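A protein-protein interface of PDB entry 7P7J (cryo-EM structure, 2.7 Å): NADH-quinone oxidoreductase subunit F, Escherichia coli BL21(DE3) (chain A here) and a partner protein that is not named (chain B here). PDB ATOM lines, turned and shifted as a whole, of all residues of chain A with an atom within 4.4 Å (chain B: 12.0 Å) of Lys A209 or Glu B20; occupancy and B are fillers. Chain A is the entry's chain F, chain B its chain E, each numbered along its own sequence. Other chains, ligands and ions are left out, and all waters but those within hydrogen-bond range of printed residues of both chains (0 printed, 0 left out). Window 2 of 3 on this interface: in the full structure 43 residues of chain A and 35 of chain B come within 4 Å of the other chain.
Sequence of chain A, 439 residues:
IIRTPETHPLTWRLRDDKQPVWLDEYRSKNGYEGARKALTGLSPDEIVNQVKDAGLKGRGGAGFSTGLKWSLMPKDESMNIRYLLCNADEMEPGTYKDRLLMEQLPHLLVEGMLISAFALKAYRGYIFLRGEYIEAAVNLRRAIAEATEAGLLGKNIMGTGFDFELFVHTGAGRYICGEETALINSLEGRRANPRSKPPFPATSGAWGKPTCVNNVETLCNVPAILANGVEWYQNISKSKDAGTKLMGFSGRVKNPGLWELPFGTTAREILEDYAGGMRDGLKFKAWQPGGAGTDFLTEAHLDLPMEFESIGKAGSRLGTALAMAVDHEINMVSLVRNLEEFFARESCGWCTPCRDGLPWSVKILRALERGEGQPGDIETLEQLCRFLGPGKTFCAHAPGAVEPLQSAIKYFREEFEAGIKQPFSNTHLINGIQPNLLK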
ATOM      1  N   ILE A  81     -12.736   1.320   3.889  1.00  0.00           N
ATOM      2  CA  ILE A  81     -11.883   0.146   3.755  1.00  0.00           C
ATOM      3  C   ILE A  81     -12.366  -0.635   2.539  1.00  0.00           C
ATOM      4  O   ILE A  81     -13.426  -1.264   2.576  1.00  0.00           O
ATOM      5  CB  ILE A  81     -11.914  -0.714   5.024  1.00  0.00           C
ATOM      6  CG1 ILE A  81     -11.350   0.072   6.208  1.00  0.00           C
ATOM      7  CG2 ILE A  81     -11.143  -2.001   4.823  1.00  0.00           C
ATOM      8  CD1 ILE A  81      -9.925   0.530   6.009  1.00  0.00           C
ATOM      9  N   TYR A  83     -11.250  -3.025  -1.151  1.00  0.00           N
ATOM     10  CA  TYR A  83     -10.289  -3.980  -1.680  1.00  0.00           C
ATOM     11  C   TYR A  83     -10.473  -4.169  -3.178  1.00  0.00           C
ATOM     12  O   TYR A  83     -11.600  -4.244  -3.681  1.00  0.00           O
ATOM     13  CB  TYR A  83     -10.412  -5.329  -0.971  1.00  0.00           C
ATOM     14  CG  TYR A  83     -10.040  -5.272   0.489  1.00  0.00           C
ATOM     15  CD1 TYR A  83      -8.713  -5.327   0.887  1.00  0.00           C
ATOM     16  CD2 TYR A  83     -11.016  -5.160   1.468  1.00  0.00           C
ATOM     17  CE1 TYR A  83      -8.368  -5.272   2.219  1.00  0.00           C
ATOM     18  CE2 TYR A  83     -10.680  -5.104   2.802  1.00  0.00           C
ATOM     19  CZ  TYR A  83      -9.356  -5.162   3.171  1.00  0.00           C
ATOM     20  OH  TYR A  83      -9.016  -5.106   4.500  1.00  0.00           O
ATOM     21  N   TYR A 123      -8.421   0.907  -0.738  1.00  0.00           N
ATOM     22  CA  TYR A 123      -7.228   1.129   0.060  1.00  0.00           C
ATOM     23  C   TYR A 123      -6.231  -0.014  -0.049  1.00  0.00           C
ATOM     24  O   TYR A 123      -5.035   0.211   0.161  1.00  0.00           O
ATOM     25  CB  TYR A 123      -7.609   1.378   1.524  1.00  0.00           C
ATOM     26  CG  TYR A 123      -7.315   0.243   2.482  1.00  0.00           C
ATOM     27  CD1 TYR A 123      -8.145  -0.868   2.555  1.00  0.00           C
ATOM     28  CD2 TYR A 123      -6.217   0.297   3.331  1.00  0.00           C
ATOM     29  CE1 TYR A 123      -7.877  -1.900   3.430  1.00  0.00           C
ATOM     30  CE2 TYR A 123      -5.946  -0.730   4.212  1.00  0.00           C
ATOM     31  CZ  TYR A 123      -6.782  -1.823   4.259  1.00  0.00           C
ATOM     32  OH  TYR A 123      -6.517  -2.849   5.133  1.00  0.00           O
ATOM     33  N   ARG A 124      -6.675  -1.230  -0.372  1.00  0.00           N
ATOM     34  CA  ARG A 124      -5.730  -2.328  -0.527  1.00  0.00           C
ATOM     35  C   ARG A 124      -6.016  -3.123  -1.792  1.00  0.00           C
ATOM     36  O   ARG A 124      -7.159  -3.210  -2.250  1.00  0.00           O
ATOM     37  CB  ARG A 124      -5.738  -3.262   0.684  1.00  0.00           C
ATOM     38  CG  ARG A 124      -4.402  -3.314   1.400  1.00  0.00           C
ATOM     39  CD  ARG A 124      -4.504  -4.021   2.733  1.00  0.00           C
ATOM     40  NE  ARG A 124      -3.317  -3.801   3.548  1.00  0.00           N
ATOM     41  CZ  ARG A 124      -3.206  -4.159   4.819  1.00  0.00           C
ATOM     42  NH1 ARG A 124      -4.199  -4.754   5.458  1.00  0.00           N
ATOM     43  NH2 ARG A 124      -2.072  -3.911   5.465  1.00  0.00           N
ATOM     44  N   PRO A 201     -20.174  -8.845  -4.254  1.00  0.00           N
ATOM     45  CA  PRO A 201     -18.903  -8.445  -3.626  1.00  0.00           C
ATOM     46  C   PRO A 201     -18.695  -6.943  -3.543  1.00  0.00           C
ATOM     47  O   PRO A 201     -17.943  -6.487  -2.673  1.00  0.00           O
ATOM     48  CB  PRO A 201     -17.856  -9.105  -4.530  1.00  0.00           C
ATOM     49  CG  PRO A 201     -18.540 -10.304  -5.055  1.00  0.00           C
ATOM     50  CD  PRO A 201     -19.972  -9.906  -5.257  1.00  0.00           C
ATOM     51  N   SER A 204     -20.429  -6.200  -0.152  1.00  0.00           N
ATOM     52  CA  SER A 204     -19.657  -6.779   0.946  1.00  0.00           C
ATOM     53  C   SER A 204     -18.893  -7.976   0.387  1.00  0.00           C
ATOM     54  O   SER A 204     -19.475  -9.043   0.177  1.00  0.00           O
ATOM     55  CB  SER A 204     -20.560  -7.183   2.102  1.00  0.00           C
ATOM     56  OG  SER A 204     -21.463  -8.198   1.705  1.00  0.00           O
ATOM     57  N   GLY A 205     -17.597  -7.791   0.152  1.00  0.00           N
ATOM     58  CA  GLY A 205     -16.777  -8.839  -0.421  1.00  0.00           C
ATOM     59  C   GLY A 205     -15.731  -9.385   0.526  1.00  0.00           C
ATOM     60  O   GLY A 205     -16.040 -10.206   1.393  1.00  0.00           O
ATOM     61  N   ALA A 206     -14.488  -8.940   0.365  1.00  0.00           N
ATOM     62  CA  ALA A 206     -13.387  -9.450   1.172  1.00  0.00           C
ATOM     63  C   ALA A 206     -13.488  -8.912   2.592  1.00  0.00           C
ATOM     64  O   ALA A 206     -13.420  -7.696   2.806  1.00  0.00           O
ATOM     65  CB  ALA A 206     -12.051  -9.066   0.545  1.00  0.00           C
ATOM     66  N   TRP A 207     -13.656  -9.828   3.552  1.00  0.00           N
ATOM     67  CA  TRP A 207     -13.807  -9.514   4.976  1.00  0.00           C
ATOM     68  C   TRP A 207     -14.975  -8.562   5.223  1.00  0.00           C
ATOM     69  O   TRP A 207     -14.909  -7.679   6.079  1.00  0.00           O
ATOM     70  CB  TRP A 207     -12.511  -8.959   5.568  1.00  0.00           C
ATOM     71  CG  TRP A 207     -11.343  -9.871   5.393  1.00  0.00           C
ATOM     72  CD1 TRP A 207     -11.092 -11.017   6.082  1.00  0.00           C
ATOM     73  CD2 TRP A 207     -10.265  -9.714   4.466  1.00  0.00           C
ATOM     74  NE1 TRP A 207      -9.924 -11.587   5.642  1.00  0.00           N
ATOM     75  CE2 TRP A 207      -9.397 -10.805   4.650  1.00  0.00           C
ATOM     76  CE3 TRP A 207      -9.950  -8.758   3.499  1.00  0.00           C
ATOM     77  CZ2 TRP A 207      -8.236 -10.967   3.902  1.00  0.00           C
ATOM     78  CZ3 TRP A 207      -8.798  -8.920   2.759  1.00  0.00           C
ATOM     79  CH2 TRP A 207      -7.956 -10.016   2.964  1.00  0.00           C
ATOM     80  N   GLY A 208     -16.051  -8.739   4.461  1.00  0.00           N
ATOM     81  CA  GLY A 208     -17.235  -7.923   4.629  1.00  0.00           C
ATOM     82  C   GLY A 208     -17.121  -6.511   4.108  1.00  0.00           C
ATOM     83  O   GLY A 208     -18.043  -5.716   4.312  1.00  0.00           O
ATOM     84  N   LYS A 209     -16.033  -6.177   3.447  1.00  0.00           N
ATOM     85  CA  LYS A 209     -15.778  -4.848   2.928  1.00  0.00           C
ATOM     86  C   LYS A 209     -16.119  -4.783   1.450  1.00  0.00           C
ATOM     87  O   LYS A 209     -16.191  -5.814   0.776  1.00  0.00           O
ATOM     88  CB  LYS A 209     -14.310  -4.471   3.141  1.00  0.00           C
ATOM     89  CG  LYS A 209     -13.840  -4.618   4.574  1.00  0.00           C
ATOM     90  CD  LYS A 209     -14.603  -3.691   5.499  1.00  0.00           C
ATOM     91  CE  LYS A 209     -14.132  -3.845   6.935  1.00  0.00           C
ATOM     92  NZ  LYS A 209     -14.329  -5.233   7.436  1.00  0.00           N
ATOM     93  N   PRO A 210     -16.389  -3.588   0.924  1.00  0.00           N
ATOM     94  CA  PRO A 210     -16.548  -3.440  -0.528  1.00  0.00           C
ATOM     95  C   PRO A 210     -15.294  -3.870  -1.278  1.00  0.00           C
ATOM     96  O   PRO A 210     -14.180  -3.416  -0.991  1.00  0.00           O
ATOM     97  CB  PRO A 210     -16.838  -1.944  -0.709  1.00  0.00           C
ATOM     98  CG  PRO A 210     -16.773  -1.333   0.663  1.00  0.00           C
ATOM     99  CD  PRO A 210     -16.913  -2.424   1.652  1.00  0.00           C
ATOM    100  N   THR A 211     -15.491  -4.763  -2.242  1.00  0.00           N
ATOM    101  CA  THR A 211     -14.398  -5.446  -2.912  1.00  0.00           C
ATOM    102  C   THR A 211     -14.773  -5.638  -4.372  1.00  0.00           C
ATOM    103  O   THR A 211     -15.881  -6.087  -4.671  1.00  0.00           O
ATOM    104  CB  THR A 211     -14.120  -6.800  -2.252  1.00  0.00           C
ATOM    105  OG1 THR A 211     -13.772  -6.598  -0.878  1.00  0.00           O
ATOM    106  CG2 THR A 211     -12.987  -7.517  -2.949  1.00  0.00           C
ATOM    107  N   ILE B  12       5.546 -16.933   8.798  1.00  0.00           N
ATOM    108  CA  ILE B  12       4.099 -17.006   8.979  1.00  0.00           C
ATOM    109  C   ILE B  12       3.567 -15.696   9.550  1.00  0.00           C
ATOM    110  O   ILE B  12       2.572 -15.151   9.062  1.00  0.00           O
ATOM    111  CB  ILE B  12       3.732 -18.209   9.866  1.00  0.00           C
ATOM    112  CG1 ILE B  12       3.825 -19.506   9.065  1.00  0.00           C
ATOM    113  CG2 ILE B  12       2.335 -18.071  10.418  1.00  0.00           C
ATOM    114  CD1 ILE B  12       3.679 -20.750   9.905  1.00  0.00           C
ATOM    115  N   GLU B  13       4.245 -15.151  10.565  1.00  0.00           N
ATOM    116  CA  GLU B  13       3.809 -13.889  11.162  1.00  0.00           C
ATOM    117  C   GLU B  13       3.945 -12.726  10.183  1.00  0.00           C
ATOM    118  O   GLU B  13       3.101 -11.818  10.163  1.00  0.00           O
ATOM    119  CB  GLU B  13       4.599 -13.616  12.440  1.00  0.00           C
ATOM    120  CG  GLU B  13       4.222 -14.524  13.596  1.00  0.00           C
ATOM    121  CD  GLU B  13       5.266 -14.537  14.695  1.00  0.00           C
ATOM    122  OE1 GLU B  13       6.254 -13.781  14.587  1.00  0.00           O
ATOM    123  OE2 GLU B  13       5.098 -15.304  15.666  1.00  0.00           O
ATOM    124  N   HIS B  14       4.996 -12.743   9.357  1.00  0.00           N
ATOM    125  CA  HIS B  14       5.137 -11.724   8.323  1.00  0.00           C
ATOM    126  C   HIS B  14       4.009 -11.817   7.303  1.00  0.00           C
ATOM    127  O   HIS B  14       3.556 -10.796   6.774  1.00  0.00           O
ATOM    128  CB  HIS B  14       6.495 -11.856   7.639  1.00  0.00           C
ATOM    129  CG  HIS B  14       6.730 -10.838   6.568  1.00  0.00           C
ATOM    130  ND1 HIS B  14       6.658  -9.483   6.804  1.00  0.00           N
ATOM    131  CD2 HIS B  14       7.029 -10.977   5.255  1.00  0.00           C
ATOM    132  CE1 HIS B  14       6.907  -8.830   5.683  1.00  0.00           C
ATOM    133  NE2 HIS B  14       7.134  -9.714   4.728  1.00  0.00           N
ATOM    134  N   GLU B  15       3.545 -13.034   7.010  1.00  0.00           N
ATOM    135  CA  GLU B  15       2.376 -13.180   6.147  1.00  0.00           C
ATOM    136  C   GLU B  15       1.100 -12.706   6.834  1.00  0.00           C
ATOM    137  O   GLU B  15       0.213 -12.160   6.170  1.00  0.00           O
ATOM    138  CB  GLU B  15       2.232 -14.629   5.689  1.00  0.00           C
ATOM    139  CG  GLU B  15       3.318 -15.062   4.723  1.00  0.00           C
ATOM    140  CD  GLU B  15       3.218 -14.364   3.380  1.00  0.00           C
ATOM    141  OE1 GLU B  15       2.089 -14.041   2.954  1.00  0.00           O
ATOM    142  OE2 GLU B  15       4.271 -14.138   2.748  1.00  0.00           O
ATOM    143  N   MET B  16       0.985 -12.916   8.150  1.00  0.00           N
ATOM    144  CA  MET B  16      -0.149 -12.366   8.897  1.00  0.00           C
ATOM    145  C   MET B  16      -0.142 -10.845   8.901  1.00  0.00           C
ATOM    146  O   MET B  16      -1.199 -10.224   9.064  1.00  0.00           O
ATOM    147  CB  MET B  16      -0.165 -12.877  10.340  1.00  0.00           C
ATOM    148  CG  MET B  16      -0.092 -14.375  10.506  1.00  0.00           C
ATOM    149  SD  MET B  16       0.144 -14.880  12.220  1.00  0.00           S
ATOM    150  CE  MET B  16      -1.089 -13.887  13.047  1.00  0.00           C
ATOM    151  N   HIS B  17       1.028 -10.225   8.736  1.00  0.00           N
ATOM    152  CA  HIS B  17       1.083  -8.770   8.647  1.00  0.00           C
ATOM    153  C   HIS B  17       0.412  -8.224   7.389  1.00  0.00           C
ATOM    154  O   HIS B  17       0.041  -7.046   7.367  1.00  0.00           O
ATOM    155  CB  HIS B  17       2.533  -8.293   8.698  1.00  0.00           C
ATOM    156  CG  HIS B  17       3.107  -8.256  10.079  1.00  0.00           C
ATOM    157  ND1 HIS B  17       4.389  -7.825  10.341  1.00  0.00           N
ATOM    158  CD2 HIS B  17       2.572  -8.594  11.276  1.00  0.00           C
ATOM    159  CE1 HIS B  17       4.620  -7.901  11.640  1.00  0.00           C
ATOM    160  NE2 HIS B  17       3.533  -8.364  12.229  1.00  0.00           N
ATOM    161  N   HIS B  18       0.242  -9.043   6.350  1.00  0.00           N
ATOM    162  CA  HIS B  18      -0.274  -8.562   5.074  1.00  0.00           C
ATOM    163  C   HIS B  18      -1.795  -8.508   5.009  1.00  0.00           C
ATOM    164  O   HIS B  18      -2.332  -7.918   4.066  1.00  0.00           O
ATOM    165  CB  HIS B  18       0.242  -9.442   3.935  1.00  0.00           C
ATOM    166  CG  HIS B  18       1.734  -9.486   3.833  1.00  0.00           C
ATOM    167  ND1 HIS B  18       2.404 -10.487   3.165  1.00  0.00           N
ATOM    168  CD2 HIS B  18       2.686  -8.653   4.314  1.00  0.00           C
ATOM    169  CE1 HIS B  18       3.704 -10.270   3.239  1.00  0.00           C
ATOM    170  NE2 HIS B  18       3.902  -9.164   3.931  1.00  0.00           N
ATOM    171  N   TYR B  19      -2.500  -9.098   5.970  1.00  0.00           N
ATOM    172  CA  TYR B  19      -3.953  -9.146   5.947  1.00  0.00           C
ATOM    173  C   TYR B  19      -4.509  -8.566   7.237  1.00  0.00           C
ATOM    174  O   TYR B  19      -3.814  -8.468   8.251  1.00  0.00           O
ATOM    175  CB  TYR B  19      -4.473 -10.575   5.761  1.00  0.00           C
ATOM    176  CG  TYR B  19      -3.794 -11.346   4.657  1.00  0.00           C
ATOM    177  CD1 TYR B  19      -4.220 -11.232   3.342  1.00  0.00           C
ATOM    178  CD2 TYR B  19      -2.736 -12.200   4.932  1.00  0.00           C
ATOM    179  CE1 TYR B  19      -3.604 -11.937   2.333  1.00  0.00           C
ATOM    180  CE2 TYR B  19      -2.115 -12.910   3.927  1.00  0.00           C
ATOM    181  CZ  TYR B  19      -2.553 -12.774   2.629  1.00  0.00           C
ATOM    182  OH  TYR B  19      -1.938 -13.478   1.622  1.00  0.00           O
ATOM    183  N   GLU B  20      -5.781  -8.183   7.188  1.00  0.00           N
ATOM    184  CA  GLU B  20      -6.471  -7.654   8.354  1.00  0.00           C
ATOM    185  C   GLU B  20      -7.081  -8.746   9.221  1.00  0.00           C
ATOM    186  O   GLU B  20      -7.642  -8.438  10.277  1.00  0.00           O
ATOM    187  CB  GLU B  20      -7.559  -6.668   7.922  1.00  0.00           C
ATOM    188  CG  GLU B  20      -8.833  -7.317   7.421  1.00  0.00           C
ATOM    189  CD  GLU B  20      -9.969  -6.326   7.292  1.00  0.00           C
ATOM    190  OE1 GLU B  20      -9.697  -5.148   6.984  1.00  0.00           O
ATOM    191  OE2 GLU B  20     -11.132  -6.716   7.515  1.00  0.00           O
ATOM    192  N   ASP B  21      -6.984 -10.009   8.804  1.00  0.00           N
ATOM    193  CA  ASP B  21      -7.497 -11.129   9.566  1.00  0.00           C
ATOM    194  C   ASP B  21      -6.396 -12.183   9.512  1.00  0.00           C
ATOM    195  O   ASP B  21      -5.894 -12.493   8.417  1.00  0.00           O
ATOM    196  CB  ASP B  21      -8.814 -11.658   8.981  1.00  0.00           C
ATOM    197  CG  ASP B  21      -9.506 -12.683   9.877  1.00  0.00           C
ATOM    198  OD1 ASP B  21     -10.734 -12.558  10.053  1.00  0.00           O
ATOM    199  OD2 ASP B  21      -8.859 -13.621  10.385  1.00  0.00           O
ATOM    200  N   PRO B  22      -5.983 -12.730  10.660  1.00  0.00           N
ATOM    201  CA  PRO B  22      -4.925 -13.755  10.653  1.00  0.00           C
ATOM    202  C   PRO B  22      -5.314 -15.057   9.971  1.00  0.00           C
ATOM    203  O   PRO B  22      -4.418 -15.835   9.627  1.00  0.00           O
ATOM    204  CB  PRO B  22      -4.643 -13.978  12.143  1.00  0.00           C
ATOM    205  CG  PRO B  22      -5.853 -13.474  12.845  1.00  0.00           C
ATOM    206  CD  PRO B  22      -6.351 -12.333  12.027  1.00  0.00           C
ATOM    207  N   ARG B  23      -6.609 -15.324   9.779  1.00  0.00           N
ATOM    208  CA  ARG B  23      -7.035 -16.541   9.093  1.00  0.00           C
ATOM    209  C   ARG B  23      -6.561 -16.564   7.645  1.00  0.00           C
ATOM    210  O   ARG B  23      -6.290 -17.639   7.096  1.00  0.00           O
ATOM    211  CB  ARG B  23      -8.560 -16.661   9.166  1.00  0.00           C
ATOM    212  CG  ARG B  23      -9.168 -17.832   8.416  1.00  0.00           C
ATOM    213  CD  ARG B  23     -10.675 -17.711   8.364  1.00  0.00           C
ATOM    214  NE  ARG B  23     -11.252 -17.667   9.701  1.00  0.00           N
ATOM    215  CZ  ARG B  23     -11.557 -18.738  10.418  1.00  0.00           C
ATOM    216  NH1 ARG B  23     -11.367 -19.960   9.951  1.00  0.00           N
ATOM    217  NH2 ARG B  23     -12.063 -18.580  11.637  1.00  0.00           N
ATOM    218  N   ALA B  24      -6.398 -15.390   7.034  1.00  0.00           N
ATOM    219  CA  ALA B  24      -6.045 -15.277   5.625  1.00  0.00           C
ATOM    220  C   ALA B  24      -4.634 -15.758   5.310  1.00  0.00           C
ATOM    221  O   ALA B  24      -4.301 -15.897   4.128  1.00  0.00           O
ATOM    222  CB  ALA B  24      -6.207 -13.831   5.170  1.00  0.00           C
ATOM    223  N   ALA B  25      -3.804 -16.012   6.317  1.00  0.00           N
ATOM    224  CA  ALA B  25      -2.456 -16.516   6.109  1.00  0.00           C
ATOM    225  C   ALA B  25      -2.360 -18.028   6.265  1.00  0.00           C
ATOM    226  O   ALA B  25      -1.251 -18.555   6.379  1.00  0.00           O
ATOM    227  CB  ALA B  25      -1.484 -15.832   7.070  1.00  0.00           C
ATOM    228  N   SER B  26      -3.493 -18.735   6.274  1.00  0.00           N
ATOM    229  CA  SER B  26      -3.468 -20.180   6.482  1.00  0.00           C
ATOM    230  C   SER B  26      -2.891 -20.913   5.279  1.00  0.00           C
ATOM    231  O   SER B  26      -2.094 -21.846   5.439  1.00  0.00           O
ATOM    232  CB  SER B  26      -4.872 -20.689   6.798  1.00  0.00           C
ATOM    233  OG  SER B  26      -5.797 -20.273   5.812  1.00  0.00           O
ATOM    234  N   LEU B  52      -1.950 -19.144  14.370  1.00  0.00           N
ATOM    235  CA  LEU B  52      -2.893 -18.245  13.717  1.00  0.00           C
ATOM    236  C   LEU B  52      -4.109 -17.910  14.569  1.00  0.00           C
ATOM    237  O   LEU B  52      -4.823 -16.955  14.248  1.00  0.00           O
ATOM    238  CB  LEU B  52      -3.366 -18.858  12.402  1.00  0.00           C
ATOM    239  CG  LEU B  52      -2.774 -18.296  11.116  1.00  0.00           C
ATOM    240  CD1 LEU B  52      -1.269 -18.361  11.140  1.00  0.00           C
ATOM    241  CD2 LEU B  52      -3.313 -19.087   9.960  1.00  0.00           C
ATOM    242  N   GLY B  53      -4.369 -18.664  15.631  1.00  0.00           N
ATOM    243  CA  GLY B  53      -5.561 -18.418  16.416  1.00  0.00           C
ATOM    244  C   GLY B  53      -6.850 -18.880  15.776  1.00  0.00           C
ATOM    245  O   GLY B  53      -7.915 -18.353  16.104  1.00  0.00           O
ATOM    246  N   ILE B  54      -6.786 -19.842  14.867  1.00  0.00           N
ATOM    247  CA  ILE B  54      -7.973 -20.402  14.226  1.00  0.00           C
ATOM    248  C   ILE B  54      -8.014 -21.884  14.573  1.00  0.00           C
ATOM    249  O   ILE B  54      -6.977 -22.477  14.913  1.00  0.00           O
ATOM    250  CB  ILE B  54      -7.974 -20.150  12.700  1.00  0.00           C
ATOM    251  CG1 ILE B  54      -6.740 -20.763  12.040  1.00  0.00           C
ATOM    252  CG2 ILE B  54      -8.055 -18.663  12.409  1.00  0.00           C
ATOM    253  CD1 ILE B  54      -6.743 -20.629  10.537  1.00  0.00           C
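The side-chain hydroxyl (OH) of Tyr A123 sits at hydrogen-bond distance from the guanidinium group (NH1) of Arg A124. The side-chain hydroxyl (OH) of Tyr A83 sits at hydrogen-bond distance from the side-chain hydroxyl (OH) of Tyr A123 (3.4 Å). N of Arg B23 sits at hydrogen-bond distance from OD2 of Asp B21 (2.9 Å). O of Lys A209 lies within hydrogen-bond range of OG1 of Thr A211 (3.0 Å). The backbone NH (N) of Tyr A83 sits at hydrogen-bond distance from the backbone carbonyl oxygen (O) of Pro A210 (3.0 Å). The backbone carbonyl oxygen of Trp A207 is in hydrogen-bond range of the side-chain amino group of Lys A209 (2.9 Å).
Arg A124 touches His B18. Tyr B19 touches Trp A207 (CD1 to CH2, 3.9 Å). OE2 of Glu B20 touches CB of Trp A207, at 3.3 Å. Asp B21 touches Trp A207 (CB to NE1, 3.5 Å). CB of Ala B24 touches CZ2 of Trp A207, 3.7 Å away.
Printed residues of chain A that touch a printed residue of chain B: Tyr A83, Arg A124, Trp A207 and Lys A209. Hydrophobic or aromatic side chains of chain A that line the printed part of chain B: Tyr A83 and Trp A207. Hydrophobic or aromatic side chains of chain B within 4 Å of the printed part of chain A: Tyr B19 and Ala B24. Along chain B the printed residues that touch a printed residue of chain A span positions 18 to 24.
Printed residues of chain B within 4 Å of Arg A124: His B18 (3.9 Å). No residue of chain B comes within 4 Å of Ser A204. No residue of chain B comes within 4 Å of Gly A205. No residue of chain B comes within 4 Å of Ala A206. Trp A207 touches just these residues of chain B: Tyr B19, Glu B20, Asp B21 and Ala B24. Of chain B, only Glu B20 comes within 4 Å of Lys A209. No residue of chain B comes within 4 Å of Pro A210. Glu B15 touches none of the printed residues of chain A. Of the printed residues of chain A, His B18 touches Arg A124. Of the printed residues of chain A, Tyr B19 touches Trp A207. Of chain A, only Tyr A83, Trp A207 and Lys A209 come within 4 Å of Glu B20. Of the printed residues of chain A, Asp B21 touches Trp A207 (3.5 Å). Of the printed residues of chain A, Ala B24 touches Trp A207. Leu B52 touches none of the printed residues of chain A. The nearest residue of chain B that does not touch Lys A209 is Asp B21 (8.6 Å). The nearest residue of chain A that does not touch Glu B20 is Ile A81 (4.1 Å).
OE1 of Glu B20 is in hydrogen-bond range of OH of Tyr A83 (2.6 Å). NZ of Lys A209 is in salt-bridge range of OE2 of Glu B20 (3.5 Å).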
